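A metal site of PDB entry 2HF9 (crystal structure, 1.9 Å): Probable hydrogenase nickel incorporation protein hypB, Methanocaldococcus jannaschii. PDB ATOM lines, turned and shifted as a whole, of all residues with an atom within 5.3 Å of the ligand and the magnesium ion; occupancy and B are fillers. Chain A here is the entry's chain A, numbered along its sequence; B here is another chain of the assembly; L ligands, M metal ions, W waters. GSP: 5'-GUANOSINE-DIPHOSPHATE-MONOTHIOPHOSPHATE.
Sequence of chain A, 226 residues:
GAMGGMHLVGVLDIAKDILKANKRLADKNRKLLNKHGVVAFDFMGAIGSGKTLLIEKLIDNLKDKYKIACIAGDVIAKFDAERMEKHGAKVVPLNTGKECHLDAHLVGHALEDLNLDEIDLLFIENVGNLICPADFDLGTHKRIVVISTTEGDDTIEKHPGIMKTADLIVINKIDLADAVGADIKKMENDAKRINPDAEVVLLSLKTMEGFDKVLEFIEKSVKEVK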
ATOM      1  N   ALA A  46      27.114 -24.294  -0.069  1.00  0.00           N
ATOM      2  CA  ALA A  46      27.429 -25.354  -1.028  1.00  0.00           C
ATOM      3  C   ALA A  46      26.578 -25.172  -2.286  1.00  0.00           C
ATOM      4  O   ALA A  46      25.769 -24.236  -2.376  1.00  0.00           O
ATOM      5  CB  ALA A  46      27.168 -26.714  -0.398  1.00  0.00           C
ATOM      6  N   ILE A  47      26.763 -26.040  -3.281  1.00  0.00           N
ATOM      7  CA  ILE A  47      25.958 -25.949  -4.503  1.00  0.00           C
ATOM      8  C   ILE A  47      24.516 -26.333  -4.192  1.00  0.00           C
ATOM      9  O   ILE A  47      24.252 -27.423  -3.671  1.00  0.00           O
ATOM     10  CB  ILE A  47      26.505 -26.855  -5.628  1.00  0.00           C
ATOM     11  CG1 ILE A  47      27.937 -26.477  -6.018  1.00  0.00           C
ATOM     12  CG2 ILE A  47      25.569 -26.821  -6.844  1.00  0.00           C
ATOM     13  CD1 ILE A  47      28.066 -25.274  -6.952  1.00  0.00           C
ATOM     14  N   GLY A  48      23.589 -25.420  -4.491  1.00  0.00           N
ATOM     15  CA  GLY A  48      22.163 -25.666  -4.357  1.00  0.00           C
ATOM     16  C   GLY A  48      21.628 -25.741  -2.931  1.00  0.00           C
ATOM     17  O   GLY A  48      20.552 -26.296  -2.713  1.00  0.00           O
ATOM     18  N   SER A  49      22.373 -25.177  -1.983  1.00  0.00           N
ATOM     19  CA  SER A  49      21.971 -25.205  -0.568  1.00  0.00           C
ATOM     20  C   SER A  49      20.660 -24.442  -0.310  1.00  0.00           C
ATOM     21  O   SER A  49      19.924 -24.762   0.629  1.00  0.00           O
ATOM     22  CB  SER A  49      23.077 -24.635   0.316  1.00  0.00           C
ATOM     23  OG  SER A  49      24.227 -25.458   0.284  1.00  0.00           O
ATOM     24  N   GLY A  50      20.392 -23.420  -1.118  1.00  0.00           N
ATOM     25  CA  GLY A  50      19.170 -22.632  -0.994  1.00  0.00           C
ATOM     26  C   GLY A  50      19.384 -21.126  -0.861  1.00  0.00           C
ATOM     27  O   GLY A  50      18.475 -20.424  -0.414  1.00  0.00           O
ATOM     28  N   LYS A  51      20.553 -20.636  -1.258  1.00  0.00           N
ATOM     29  CA  LYS A  51      20.908 -19.218  -1.134  1.00  0.00           C
ATOM     30  C   LYS A  51      19.922 -18.304  -1.850  1.00  0.00           C
ATOM     31  O   LYS A  51      19.435 -17.327  -1.285  1.00  0.00           O
ATOM     32  CB  LYS A  51      22.333 -18.940  -1.662  1.00  0.00           C
ATOM     33  CG  LYS A  51      23.451 -19.724  -0.985  1.00  0.00           C
ATOM     34  CD  LYS A  51      24.845 -19.312  -1.520  1.00  0.00           C
ATOM     35  CE  LYS A  51      25.128 -19.823  -2.936  1.00  0.00           C
ATOM     36  NZ  LYS A  51      24.959 -21.291  -3.063  1.00  0.00           N
ATOM     37  N   THR A  52      19.627 -18.627  -3.113  1.00  0.00           N
ATOM     38  CA  THR A  52      18.738 -17.782  -3.908  1.00  0.00           C
ATOM     39  C   THR A  52      17.310 -17.800  -3.357  1.00  0.00           C
ATOM     40  O   THR A  52      16.706 -16.744  -3.202  1.00  0.00           O
ATOM     41  CB  THR A  52      18.756 -18.163  -5.389  1.00  0.00           C
ATOM     42  OG1 THR A  52      20.088 -18.053  -5.883  1.00  0.00           O
ATOM     43  CG2 THR A  52      17.852 -17.220  -6.202  1.00  0.00           C
ATOM     44  N   LEU A  53      16.798 -18.983  -3.057  1.00  0.00           N
ATOM     45  CA  LEU A  53      15.460 -19.105  -2.477  1.00  0.00           C
ATOM     46  C   LEU A  53      15.352 -18.325  -1.157  1.00  0.00           C
ATOM     47  O   LEU A  53      14.336 -17.685  -0.906  1.00  0.00           O
ATOM     48  CB  LEU A  53      15.052 -20.561  -2.299  1.00  0.00           C
ATOM     49  CG  LEU A  53      13.576 -20.838  -1.986  1.00  0.00           C
ATOM     50  CD1 LEU A  53      12.622 -20.147  -2.963  1.00  0.00           C
ATOM     51  CD2 LEU A  53      13.320 -22.336  -1.968  1.00  0.00           C
ATOM     52  N   LEU A  54      16.393 -18.390  -0.334  1.00  0.00           N
ATOM     53  CA  LEU A  54      16.441 -17.617   0.910  1.00  0.00           C
ATOM     54  C   LEU A  54      16.412 -16.118   0.634  1.00  0.00           C
ATOM     55  O   LEU A  54      15.646 -15.378   1.268  1.00  0.00           O
ATOM     56  CB  LEU A  54      17.682 -17.973   1.738  1.00  0.00           C
ATOM     57  CG  LEU A  54      17.890 -17.216   3.059  1.00  0.00           C
ATOM     58  CD1 LEU A  54      16.707 -17.381   4.011  1.00  0.00           C
ATOM     59  CD2 LEU A  54      19.197 -17.643   3.734  1.00  0.00           C
ATOM     60  N   ASP A  74      27.930 -15.783 -10.095  1.00  0.00           N
ATOM     61  CA  ASP A  74      28.075 -17.194 -10.464  1.00  0.00           C
ATOM     62  C   ASP A  74      28.680 -17.273 -11.856  1.00  0.00           C
ATOM     63  O   ASP A  74      28.814 -16.251 -12.525  1.00  0.00           O
ATOM     64  CB  ASP A  74      26.735 -17.928 -10.414  1.00  0.00           C
ATOM     65  CG  ASP A  74      26.876 -19.436 -10.307  1.00  0.00           C
ATOM     66  OD1 ASP A  74      27.996 -19.949 -10.069  1.00  0.00           O
ATOM     67  OD2 ASP A  74      25.861 -20.138 -10.469  1.00  0.00           O
ATOM     68  N   ASP A  80      20.252 -16.585 -11.378  1.00  0.00           N
ATOM     69  CA  ASP A  80      19.859 -16.069 -10.068  1.00  0.00           C
ATOM     70  C   ASP A  80      19.528 -14.580 -10.081  1.00  0.00           C
ATOM     71  O   ASP A  80      18.671 -14.137  -9.316  1.00  0.00           O
ATOM     72  CB  ASP A  80      20.941 -16.371  -9.039  1.00  0.00           C
ATOM     73  CG  ASP A  80      21.062 -17.859  -8.758  1.00  0.00           C
ATOM     74  OD1 ASP A  80      20.233 -18.644  -9.256  1.00  0.00           O
ATOM     75  OD2 ASP A  80      21.994 -18.236  -8.022  1.00  0.00           O
ATOM     76  N   ARG A  83      15.939 -14.324 -11.146  1.00  0.00           N
ATOM     77  CA  ARG A  83      15.101 -14.714 -10.011  1.00  0.00           C
ATOM     78  C   ARG A  83      14.921 -13.580  -9.005  1.00  0.00           C
ATOM     79  O   ARG A  83      13.806 -13.308  -8.575  1.00  0.00           O
ATOM     80  CB  ARG A  83      15.643 -15.981  -9.332  1.00  0.00           C
ATOM     81  CG  ARG A  83      15.194 -17.281 -10.000  1.00  0.00           C
ATOM     82  CD  ARG A  83      15.933 -18.508  -9.475  1.00  0.00           C
ATOM     83  NE  ARG A  83      15.526 -18.879  -8.121  1.00  0.00           N
ATOM     84  CZ  ARG A  83      16.026 -19.913  -7.444  1.00  0.00           C
ATOM     85  NH1 ARG A  83      16.968 -20.680  -7.976  1.00  0.00           N
ATOM     86  NH2 ARG A  83      15.597 -20.169  -6.211  1.00  0.00           N
ATOM     87  N   GLU A 125      24.933 -12.788  -3.195  1.00  0.00           N
ATOM     88  CA  GLU A 125      25.048 -14.236  -3.325  1.00  0.00           C
ATOM     89  C   GLU A 125      26.405 -14.609  -3.885  1.00  0.00           C
ATOM     90  O   GLU A 125      26.701 -14.370  -5.060  1.00  0.00           O
ATOM     91  CB  GLU A 125      23.933 -14.845  -4.180  1.00  0.00           C
ATOM     92  CG  GLU A 125      23.991 -16.375  -4.187  1.00  0.00           C
ATOM     93  CD  GLU A 125      22.767 -17.021  -4.782  1.00  0.00           C
ATOM     94  OE1 GLU A 125      21.708 -16.374  -4.824  1.00  0.00           O
ATOM     95  OE2 GLU A 125      22.860 -18.190  -5.217  1.00  0.00           O
ATOM     96  N   GLY A 128      28.794 -20.782  -5.179  1.00  0.00           N
ATOM     97  CA  GLY A 128      28.566 -21.996  -4.385  1.00  0.00           C
ATOM     98  C   GLY A 128      29.826 -22.816  -4.215  1.00  0.00           C
ATOM     99  O   GLY A 128      30.251 -23.512  -5.142  1.00  0.00           O
ATOM    100  N   ASN A 172      19.553 -25.688   6.093  1.00  0.00           N
ATOM    101  CA  ASN A 172      18.355 -25.607   5.282  1.00  0.00           C
ATOM    102  C   ASN A 172      17.866 -26.991   4.856  1.00  0.00           C
ATOM    103  O   ASN A 172      18.562 -27.995   5.067  1.00  0.00           O
ATOM    104  CB  ASN A 172      18.610 -24.707   4.047  1.00  0.00           C
ATOM    105  CG  ASN A 172      17.349 -24.361   3.277  1.00  0.00           C
ATOM    106  OD1 ASN A 172      17.356 -24.303   2.042  1.00  0.00           O
ATOM    107  ND2 ASN A 172      16.254 -24.133   3.998  1.00  0.00           N
ATOM    108  N   LYS A 173      16.667 -27.041   4.278  1.00  0.00           N
ATOM    109  CA  LYS A 173      16.023 -28.279   3.789  1.00  0.00           C
ATOM    110  C   LYS A 173      15.776 -29.290   4.912  1.00  0.00           C
ATOM    111  O   LYS A 173      15.910 -30.495   4.712  1.00  0.00           O
ATOM    112  CB  LYS A 173      16.832 -28.926   2.655  1.00  0.00           C
ATOM    113  CG  LYS A 173      17.059 -28.028   1.437  1.00  0.00           C
ATOM    114  CD  LYS A 173      17.779 -28.777   0.321  1.00  0.00           C
ATOM    115  CE  LYS A 173      18.372 -27.801  -0.677  1.00  0.00           C
ATOM    116  NZ  LYS A 173      19.532 -28.422  -1.409  1.00  0.00           N
ATOM    117  N   ILE A 174      15.393 -28.807   6.090  1.00  0.00           N
ATOM    118  CA  ILE A 174      15.133 -29.711   7.221  1.00  0.00           C
ATOM    119  C   ILE A 174      13.957 -30.657   6.936  1.00  0.00           C
ATOM    120  O   ILE A 174      13.855 -31.722   7.543  1.00  0.00           O
ATOM    121  CB  ILE A 174      14.948 -28.977   8.584  1.00  0.00           C
ATOM    122  CG1 ILE A 174      13.736 -28.038   8.572  1.00  0.00           C
ATOM    123  CG2 ILE A 174      16.264 -28.263   8.984  1.00  0.00           C
ATOM    124  CD1 ILE A 174      13.361 -27.464   9.950  1.00  0.00           C
ATOM    125  N   ASP A 175      13.107 -30.273   5.990  1.00  0.00           N
ATOM    126  CA  ASP A 175      11.998 -31.106   5.550  1.00  0.00           C
ATOM    127  C   ASP A 175      12.453 -32.376   4.819  1.00  0.00           C
ATOM    128  O   ASP A 175      11.675 -33.314   4.654  1.00  0.00           O
ATOM    129  CB  ASP A 175      11.015 -30.300   4.691  1.00  0.00           C
ATOM    130  CG  ASP A 175      11.656 -29.700   3.445  1.00  0.00           C
ATOM    131  OD1 ASP A 175      12.465 -28.745   3.564  1.00  0.00           O
ATOM    132  OD2 ASP A 175      11.335 -30.178   2.342  1.00  0.00           O
ATOM    133  N   LEU A 176      13.729 -32.421   4.412  1.00  0.00           N
ATOM    134  CA  LEU A 176      14.266 -33.562   3.654  1.00  0.00           C
ATOM    135  C   LEU A 176      15.252 -34.432   4.436  1.00  0.00           C
ATOM    136  O   LEU A 176      15.834 -35.364   3.880  1.00  0.00           O
ATOM    137  CB  LEU A 176      14.933 -33.061   2.365  1.00  0.00           C
ATOM    138  CG  LEU A 176      14.106 -32.155   1.447  1.00  0.00           C
ATOM    139  CD1 LEU A 176      14.955 -31.635   0.304  1.00  0.00           C
ATOM    140  CD2 LEU A 176      12.887 -32.879   0.916  1.00  0.00           C
ATOM    141  N   LEU A 203      16.240 -24.548   9.209  1.00  0.00           N
ATOM    142  CA  LEU A 203      15.335 -23.920   8.258  1.00  0.00           C
ATOM    143  C   LEU A 203      14.769 -24.878   7.225  1.00  0.00           C
ATOM    144  O   LEU A 203      15.453 -25.790   6.767  1.00  0.00           O
ATOM    145  CB  LEU A 203      16.061 -22.758   7.531  1.00  0.00           C
ATOM    146  CG  LEU A 203      15.277 -21.942   6.491  1.00  0.00           C
ATOM    147  CD1 LEU A 203      14.149 -21.153   7.126  1.00  0.00           C
ATOM    148  CD2 LEU A 203      16.202 -21.025   5.701  1.00  0.00           C
ATOM    149  N   SER A 204      13.504 -24.662   6.881  1.00  0.00           N
ATOM    150  CA  SER A 204      12.950 -25.198   5.649  1.00  0.00           C
ATOM    151  C   SER A 204      12.328 -24.052   4.875  1.00  0.00           C
ATOM    152  O   SER A 204      11.397 -23.402   5.371  1.00  0.00           O
ATOM    153  CB  SER A 204      11.903 -26.274   5.918  1.00  0.00           C
ATOM    154  OG  SER A 204      11.261 -26.638   4.699  1.00  0.00           O
ATOM    155  N   LEU A 205      12.836 -23.803   3.675  1.00  0.00           N
ATOM    156  CA  LEU A 205      12.239 -22.792   2.796  1.00  0.00           C
ATOM    157  C   LEU A 205      11.000 -23.316   2.070  1.00  0.00           C
ATOM    158  O   LEU A 205      10.357 -22.573   1.323  1.00  0.00           O
ATOM    159  CB  LEU A 205      13.283 -22.249   1.820  1.00  0.00           C
ATOM    160  CG  LEU A 205      14.336 -21.353   2.475  1.00  0.00           C
ATOM    161  CD1 LEU A 205      15.539 -21.161   1.564  1.00  0.00           C
ATOM    162  CD2 LEU A 205      13.734 -19.993   2.899  1.00  0.00           C
ATOM    163  N   LYS A 206      10.691 -24.590   2.275  1.00  0.00           N
ATOM    164  CA  LYS A 206       9.458 -25.197   1.757  1.00  0.00           C
ATOM    165  C   LYS A 206       8.301 -24.982   2.749  1.00  0.00           C
ATOM    166  O   LYS A 206       7.261 -24.446   2.378  1.00  0.00           O
ATOM    167  CB  LYS A 206       9.674 -26.685   1.470  1.00  0.00           C
ATOM    168  CG  LYS A 206       8.488 -27.399   0.821  1.00  0.00           C
ATOM    169  CD  LYS A 206       8.900 -28.801   0.378  1.00  0.00           C
ATOM    170  CE  LYS A 206       7.878 -29.444  -0.539  1.00  0.00           C
ATOM    171  NZ  LYS A 206       8.433 -30.703  -1.130  1.00  0.00           N
ATOM    172  N   THR B 150      18.873 -32.593  -5.681  1.00  0.00           N
ATOM    173  CA  THR B 150      18.657 -31.679  -4.543  1.00  0.00           C
ATOM    174  C   THR B 150      19.462 -30.375  -4.642  1.00  0.00           C
ATOM    175  O   THR B 150      19.228 -29.438  -3.886  1.00  0.00           O
ATOM    176  CB  THR B 150      18.879 -32.362  -3.175  1.00  0.00           C
ATOM    177  OG1 THR B 150      20.196 -32.948  -3.112  1.00  0.00           O
ATOM    178  CG2 THR B 150      17.828 -33.442  -2.942  1.00  0.00           C
ATOM    179  N   GLU B 151      20.401 -30.327  -5.591  1.00  0.00           N
ATOM    180  CA  GLU B 151      21.144 -29.103  -5.883  1.00  0.00           C
ATOM    181  C   GLU B 151      20.336 -28.129  -6.773  1.00  0.00           C
ATOM    182  O   GLU B 151      20.736 -26.986  -6.985  1.00  0.00           O
ATOM    183  CB  GLU B 151      22.484 -29.456  -6.532  1.00  0.00           C
ATOM    184  CG  GLU B 151      23.447 -30.163  -5.587  1.00  0.00           C
ATOM    185  CD  GLU B 151      24.258 -31.273  -6.261  1.00  0.00           C
ATOM    186  OE1 GLU B 151      24.520 -31.187  -7.478  1.00  0.00           O
ATOM    187  OE2 GLU B 151      24.645 -32.245  -5.561  1.00  0.00           O
ATOM    188  N   GLY B 152      19.193 -28.603  -7.261  1.00  0.00           N
ATOM    189  CA  GLY B 152      18.369 -27.815  -8.190  1.00  0.00           C
ATOM    190  C   GLY B 152      18.621 -28.242  -9.626  1.00  0.00           C
ATOM    191  O   GLY B 152      19.745 -28.636  -9.969  1.00  0.00           O
ATOM    192  N   ASP B 153      17.592 -28.154 -10.465  1.00  0.00           N
ATOM    193  CA  ASP B 153      17.690 -28.684 -11.833  1.00  0.00           C
ATOM    194  C   ASP B 153      18.412 -27.772 -12.826  1.00  0.00           C
ATOM    195  O   ASP B 153      18.462 -28.067 -14.024  1.00  0.00           O
ATOM    196  CB  ASP B 153      16.319 -29.143 -12.371  1.00  0.00           C
ATOM    197  CG  ASP B 153      15.284 -28.033 -12.401  1.00  0.00           C
ATOM    198  OD1 ASP B 153      15.648 -26.832 -12.338  1.00  0.00           O
ATOM    199  OD2 ASP B 153      14.091 -28.361 -12.500  1.00  0.00           O
ATOM    200  N   LYS B 158      24.285 -24.573 -15.264  1.00  0.00           N
ATOM    201  CA  LYS B 158      25.068 -23.540 -14.556  1.00  0.00           C
ATOM    202  C   LYS B 158      26.575 -23.828 -14.511  1.00  0.00           C
ATOM    203  O   LYS B 158      27.365 -22.935 -14.190  1.00  0.00           O
ATOM    204  CB  LYS B 158      24.561 -23.371 -13.134  1.00  0.00           C
ATOM    205  CG  LYS B 158      23.295 -22.560 -13.001  1.00  0.00           C
ATOM    206  CD  LYS B 158      22.828 -22.557 -11.554  1.00  0.00           C
ATOM    207  CE  LYS B 158      21.745 -21.538 -11.332  1.00  0.00           C
ATOM    208  NZ  LYS B 158      21.524 -21.325  -9.870  1.00  0.00           N
ATOM    209  N   HIS B 159      26.970 -25.057 -14.810  1.00  0.00           N
ATOM    210  CA  HIS B 159      28.372 -25.451 -14.722  1.00  0.00           C
ATOM    211  C   HIS B 159      28.840 -26.244 -15.933  1.00  0.00           C
ATOM    212  O   HIS B 159      29.317 -27.378 -15.798  1.00  0.00           O
ATOM    213  CB  HIS B 159      28.635 -26.219 -13.417  1.00  0.00           C
ATOM    214  CG  HIS B 159      28.155 -25.502 -12.194  1.00  0.00           C
ATOM    215  ND1 HIS B 159      26.883 -25.691 -11.685  1.00  0.00           N
ATOM    216  CD2 HIS B 159      28.744 -24.572 -11.407  1.00  0.00           C
ATOM    217  CE1 HIS B 159      26.729 -24.913 -10.616  1.00  0.00           C
ATOM    218  NE2 HIS B 159      27.844 -24.227 -10.440  1.00  0.00           N
ATOM    219  N   ALA B 179      10.461 -33.622  -4.266  1.00  0.00           N
ATOM    220  CA  ALA B 179      10.539 -32.883  -3.012  1.00  0.00           C
ATOM    221  C   ALA B 179      11.244 -31.522  -3.139  1.00  0.00           C
ATOM    222  O   ALA B 179      10.922 -30.581  -2.416  1.00  0.00           O
ATOM    223  CB  ALA B 179      11.201 -33.735  -1.937  1.00  0.00           C
ATOM    224  N   VAL B 180      12.206 -31.424  -4.069  1.00  0.00           N
ATOM    225  CA  VAL B 180      12.888 -30.149  -4.345  1.00  0.00           C
ATOM    226  C   VAL B 180      12.335 -29.426  -5.577  1.00  0.00           C
ATOM    227  O   VAL B 180      12.768 -28.307  -5.888  1.00  0.00           O
ATOM    228  CB  VAL B 180      14.438 -30.338  -4.502  1.00  0.00           C
ATOM    229  CG1 VAL B 180      15.094 -30.564  -3.148  1.00  0.00           C
ATOM    230  CG2 VAL B 180      14.768 -31.472  -5.466  1.00  0.00           C
ATOM    231  N   GLY B 181      11.404 -30.057  -6.272  1.00  0.00           N
ATOM    232  CA  GLY B 181      10.806 -29.482  -7.473  1.00  0.00           C
ATOM    233  C   GLY B 181      11.697 -29.587  -8.710  1.00  0.00           C
ATOM    234  O   GLY B 181      11.455 -28.905  -9.710  1.00  0.00           O
ATOM    235  N   ALA B 182      12.729 -30.424  -8.639  1.00  0.00           N
ATOM    236  CA  ALA B 182      13.650 -30.639  -9.766  1.00  0.00           C
ATOM    237  C   ALA B 182      13.009 -31.425 -10.913  1.00  0.00           C
ATOM    238  O   ALA B 182      12.345 -32.443 -10.690  1.00  0.00           O
ATOM    239  CB  ALA B 182      14.904 -31.331  -9.295  1.00  0.00           C
HETATM  240  PG  GSP L   1      23.234 -22.158  -6.569  1.00  0.00           P
HETATM  241  O3B GSP L   1      22.078 -22.784  -5.639  1.00  0.00           O
HETATM  242  S1G GSP L   1      24.778 -22.614  -5.944  1.00  0.00           S
HETATM  243  O2G GSP L   1      23.030 -22.749  -7.971  1.00  0.00           O
HETATM  244  O3G GSP L   1      23.075 -20.626  -6.616  1.00  0.00           O
HETATM  245  PB  GSP L   1      21.358 -22.018  -4.424  1.00  0.00           P
HETATM  246  O1B GSP L   1      22.135 -22.257  -3.187  1.00  0.00           O
HETATM  247  O2B GSP L   1      21.128 -20.582  -4.680  1.00  0.00           O
HETATM  248  PA  GSP L   1      18.531 -22.583  -4.822  1.00  0.00           P
HETATM  249  O1A GSP L   1      17.883 -21.442  -4.116  1.00  0.00           O
HETATM  250  O2A GSP L   1      18.538 -22.394  -6.289  1.00  0.00           O
HETATM  251  O3A GSP L   1      20.001 -22.877  -4.248  1.00  0.00           O
HETATM  252  O5' GSP L   1      17.787 -23.933  -4.373  1.00  0.00           O
HETATM  253  C5' GSP L   1      18.215 -25.193  -4.843  1.00  0.00           C
HETATM  254  C4' GSP L   1      17.037 -26.160  -4.888  1.00  0.00           C
HETATM  255  O4' GSP L   1      16.642 -26.520  -3.576  1.00  0.00           O
HETATM  256  C3' GSP L   1      15.810 -25.579  -5.555  1.00  0.00           C
HETATM  257  O3' GSP L   1      15.244 -26.637  -6.307  1.00  0.00           O
HETATM  258  C2' GSP L   1      14.898 -25.202  -4.411  1.00  0.00           C
HETATM  259  O2' GSP L   1      13.541 -25.312  -4.740  1.00  0.00           O
HETATM  260  C1' GSP L   1      15.276 -26.240  -3.365  1.00  0.00           C
HETATM  261  N9  GSP L   1      15.139 -25.830  -1.954  1.00  0.00           N
HETATM  262  C8  GSP L   1      15.741 -24.776  -1.316  1.00  0.00           C
HETATM  263  N7  GSP L   1      15.379 -24.821  -0.009  1.00  0.00           N
HETATM  264  C5  GSP L   1      14.592 -25.903   0.192  1.00  0.00           C
HETATM  265  C6  GSP L   1      13.966 -26.415   1.317  1.00  0.00           C
HETATM  266  O6  GSP L   1      14.081 -25.858   2.407  1.00  0.00           O
HETATM  267  N1  GSP L   1      13.203 -27.570   1.205  1.00  0.00           N
HETATM  268  C2  GSP L   1      13.073 -28.202  -0.030  1.00  0.00           C
HETATM  269  N2  GSP L   1      12.339 -29.300  -0.134  1.00  0.00           N
HETATM  270  N3  GSP L   1      13.700 -27.684  -1.142  1.00  0.00           N
HETATM  271  C4  GSP L   1      14.449 -26.555  -1.027  1.00  0.00           C
HETATM  272 MG    MG M   1      21.543 -19.455  -6.334  1.00  0.00          MG
HETATM  273  O   HOH W   1      20.259 -20.616  -7.422  1.00  0.00           O
HETATM  274  O   HOH W   2      11.314 -26.636  -3.048  1.00  0.00           O
HETATM  275  O   HOH W   3      15.227 -27.141  -9.167  1.00  0.00           O
HETATM  276  O   HOH W   4      23.708 -25.038  -9.301  1.00  0.00           O
HETATM  277  O   HOH W   5      13.410 -22.670  -5.989  1.00  0.00           O
HETATM  278  O   HOH W   6      26.010 -22.444  -9.008  1.00  0.00           O
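The backbone NH of Thr 52 is in hydrogen-bond range of an oxygen (O1A) of the ligand.
N of Leu 205 lies within hydrogen-bond range of O6 of the ligand, at 2.7 Å.
A nitrogen (N1) of the ligand lies within hydrogen-bond range of the side-chain carboxylate of Asp 175.
The side-chain amino group (NZ) of Lys 158 of chain B lies within hydrogen-bond range of an oxygen (O2G) of the ligand (2.8 Å).
O2A of the ligand lies within salt-bridge range of NH1 of Arg 83 (2.9 Å).
The backbone NH (N) of Leu 53 is in hydrogen-bond range of an oxygen (O1A) of the ligand (2.9 Å).
The side-chain amide oxygen of Asn 172 lies close to a nitrogen (N7) of the ligand, at 2.9 Å.
N of Gly 50 sits at hydrogen-bond distance from O1B of the ligand (2.9 Å).
An oxygen (O1B) of the ligand lies within hydrogen-bond range of the backbone NH (N) of Lys 51, 3.0 Å away.
The side-chain amino group of Lys 51 is in salt-bridge range of an oxygen (O1B) of the ligand, 3.0 Å away.
The backbone carbonyl oxygen (O) of Ala 179 of chain B lies within hydrogen-bond range of a nitrogen (N2) of the ligand, 3.0 Å away.
O of Val 180 of chain B sits at hydrogen-bond distance from O3' of the ligand (3.0 Å).
The backbone NH (N) of Gly 48 sits close to an oxygen (O3B) of the ligand (3.2 Å).
The backbone NH (N) of Ser 49 is in hydrogen-bond range of an oxygen (O1B) of the ligand (3.2 Å).
N of Lys 173 sits close to O6 of the ligand.
The side-chain carboxylate (OD1) of Asp 80 is in salt-bridge range of the side-chain amino group (NZ) of Lys 158 of chain B (3.0 Å).
The side-chain amide oxygen of Asn 172 sits close to the backbone carbonyl oxygen of Ser 49 (3.0 Å).
ND2 of Asn 172 sits close to O of Leu 203, 3.3 Å away.
O of Ala 179 of chain B sits at hydrogen-bond distance from NZ of Lys 206 (2.8 Å).
O of Gly 48 lies within hydrogen-bond range of NZ of Lys 173, at 2.7 Å.
OG of Ser 49 is in hydrogen-bond range of N of Ala 46, at 3.1 Å.
The side-chain amino group (NZ) of Lys 173 lies within hydrogen-bond range of the backbone carbonyl oxygen (O) of Thr 150 of chain B (2.7 Å).
N of Lys 173 is in hydrogen-bond range of O of Leu 203 (3.0 Å).
Merely in contact with the ligand: Ile 47, Leu 176, Ser 204, Lys 206, Thr 150 of chain B, Glu 151 of chain B and Gly 152 of chain B.
Within 4 Å of the magnesium ion: Thr 52, Asp 80 and Glu 125.
The nearest printed residue that does not touch the magnesium ion is Lys 158 of chain B (4.0001 Å).
O3G of the ligand binds the magnesium ion, at 1.9 Å.
An oxygen (O2B) of the ligand binds the magnesium ion, 2.0 Å away.
Water W1 is bound to the magnesium ion, 2.0 Å away.
The magnesium ion is bound by OG1 of Thr 52 (2.1 Å).
OD2 of Asp 80 is bound to the magnesium ion, 2.1 Å away.
OE2 of Glu 125 binds the magnesium ion, 2.1 Å away.
Water W1 lies within hydrogen-bond range of OD1 of Asp 80, O2A of the ligand, NZ of Lys 158 of chain B and NH1 of Arg 83.
Water W3 lies within hydrogen-bond range of N of Asp 153 of chain B and O3' of the ligand.
Water W5 lies within hydrogen-bond range of O2' of the ligand and NH2 of Arg 83.
Water W6 lies within hydrogen-bond range of OD2 of Asp 74 (2.7 Å), NE2 of His 159 of chain B (2.9 Å) and O2G of the ligand (3.2 Å).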
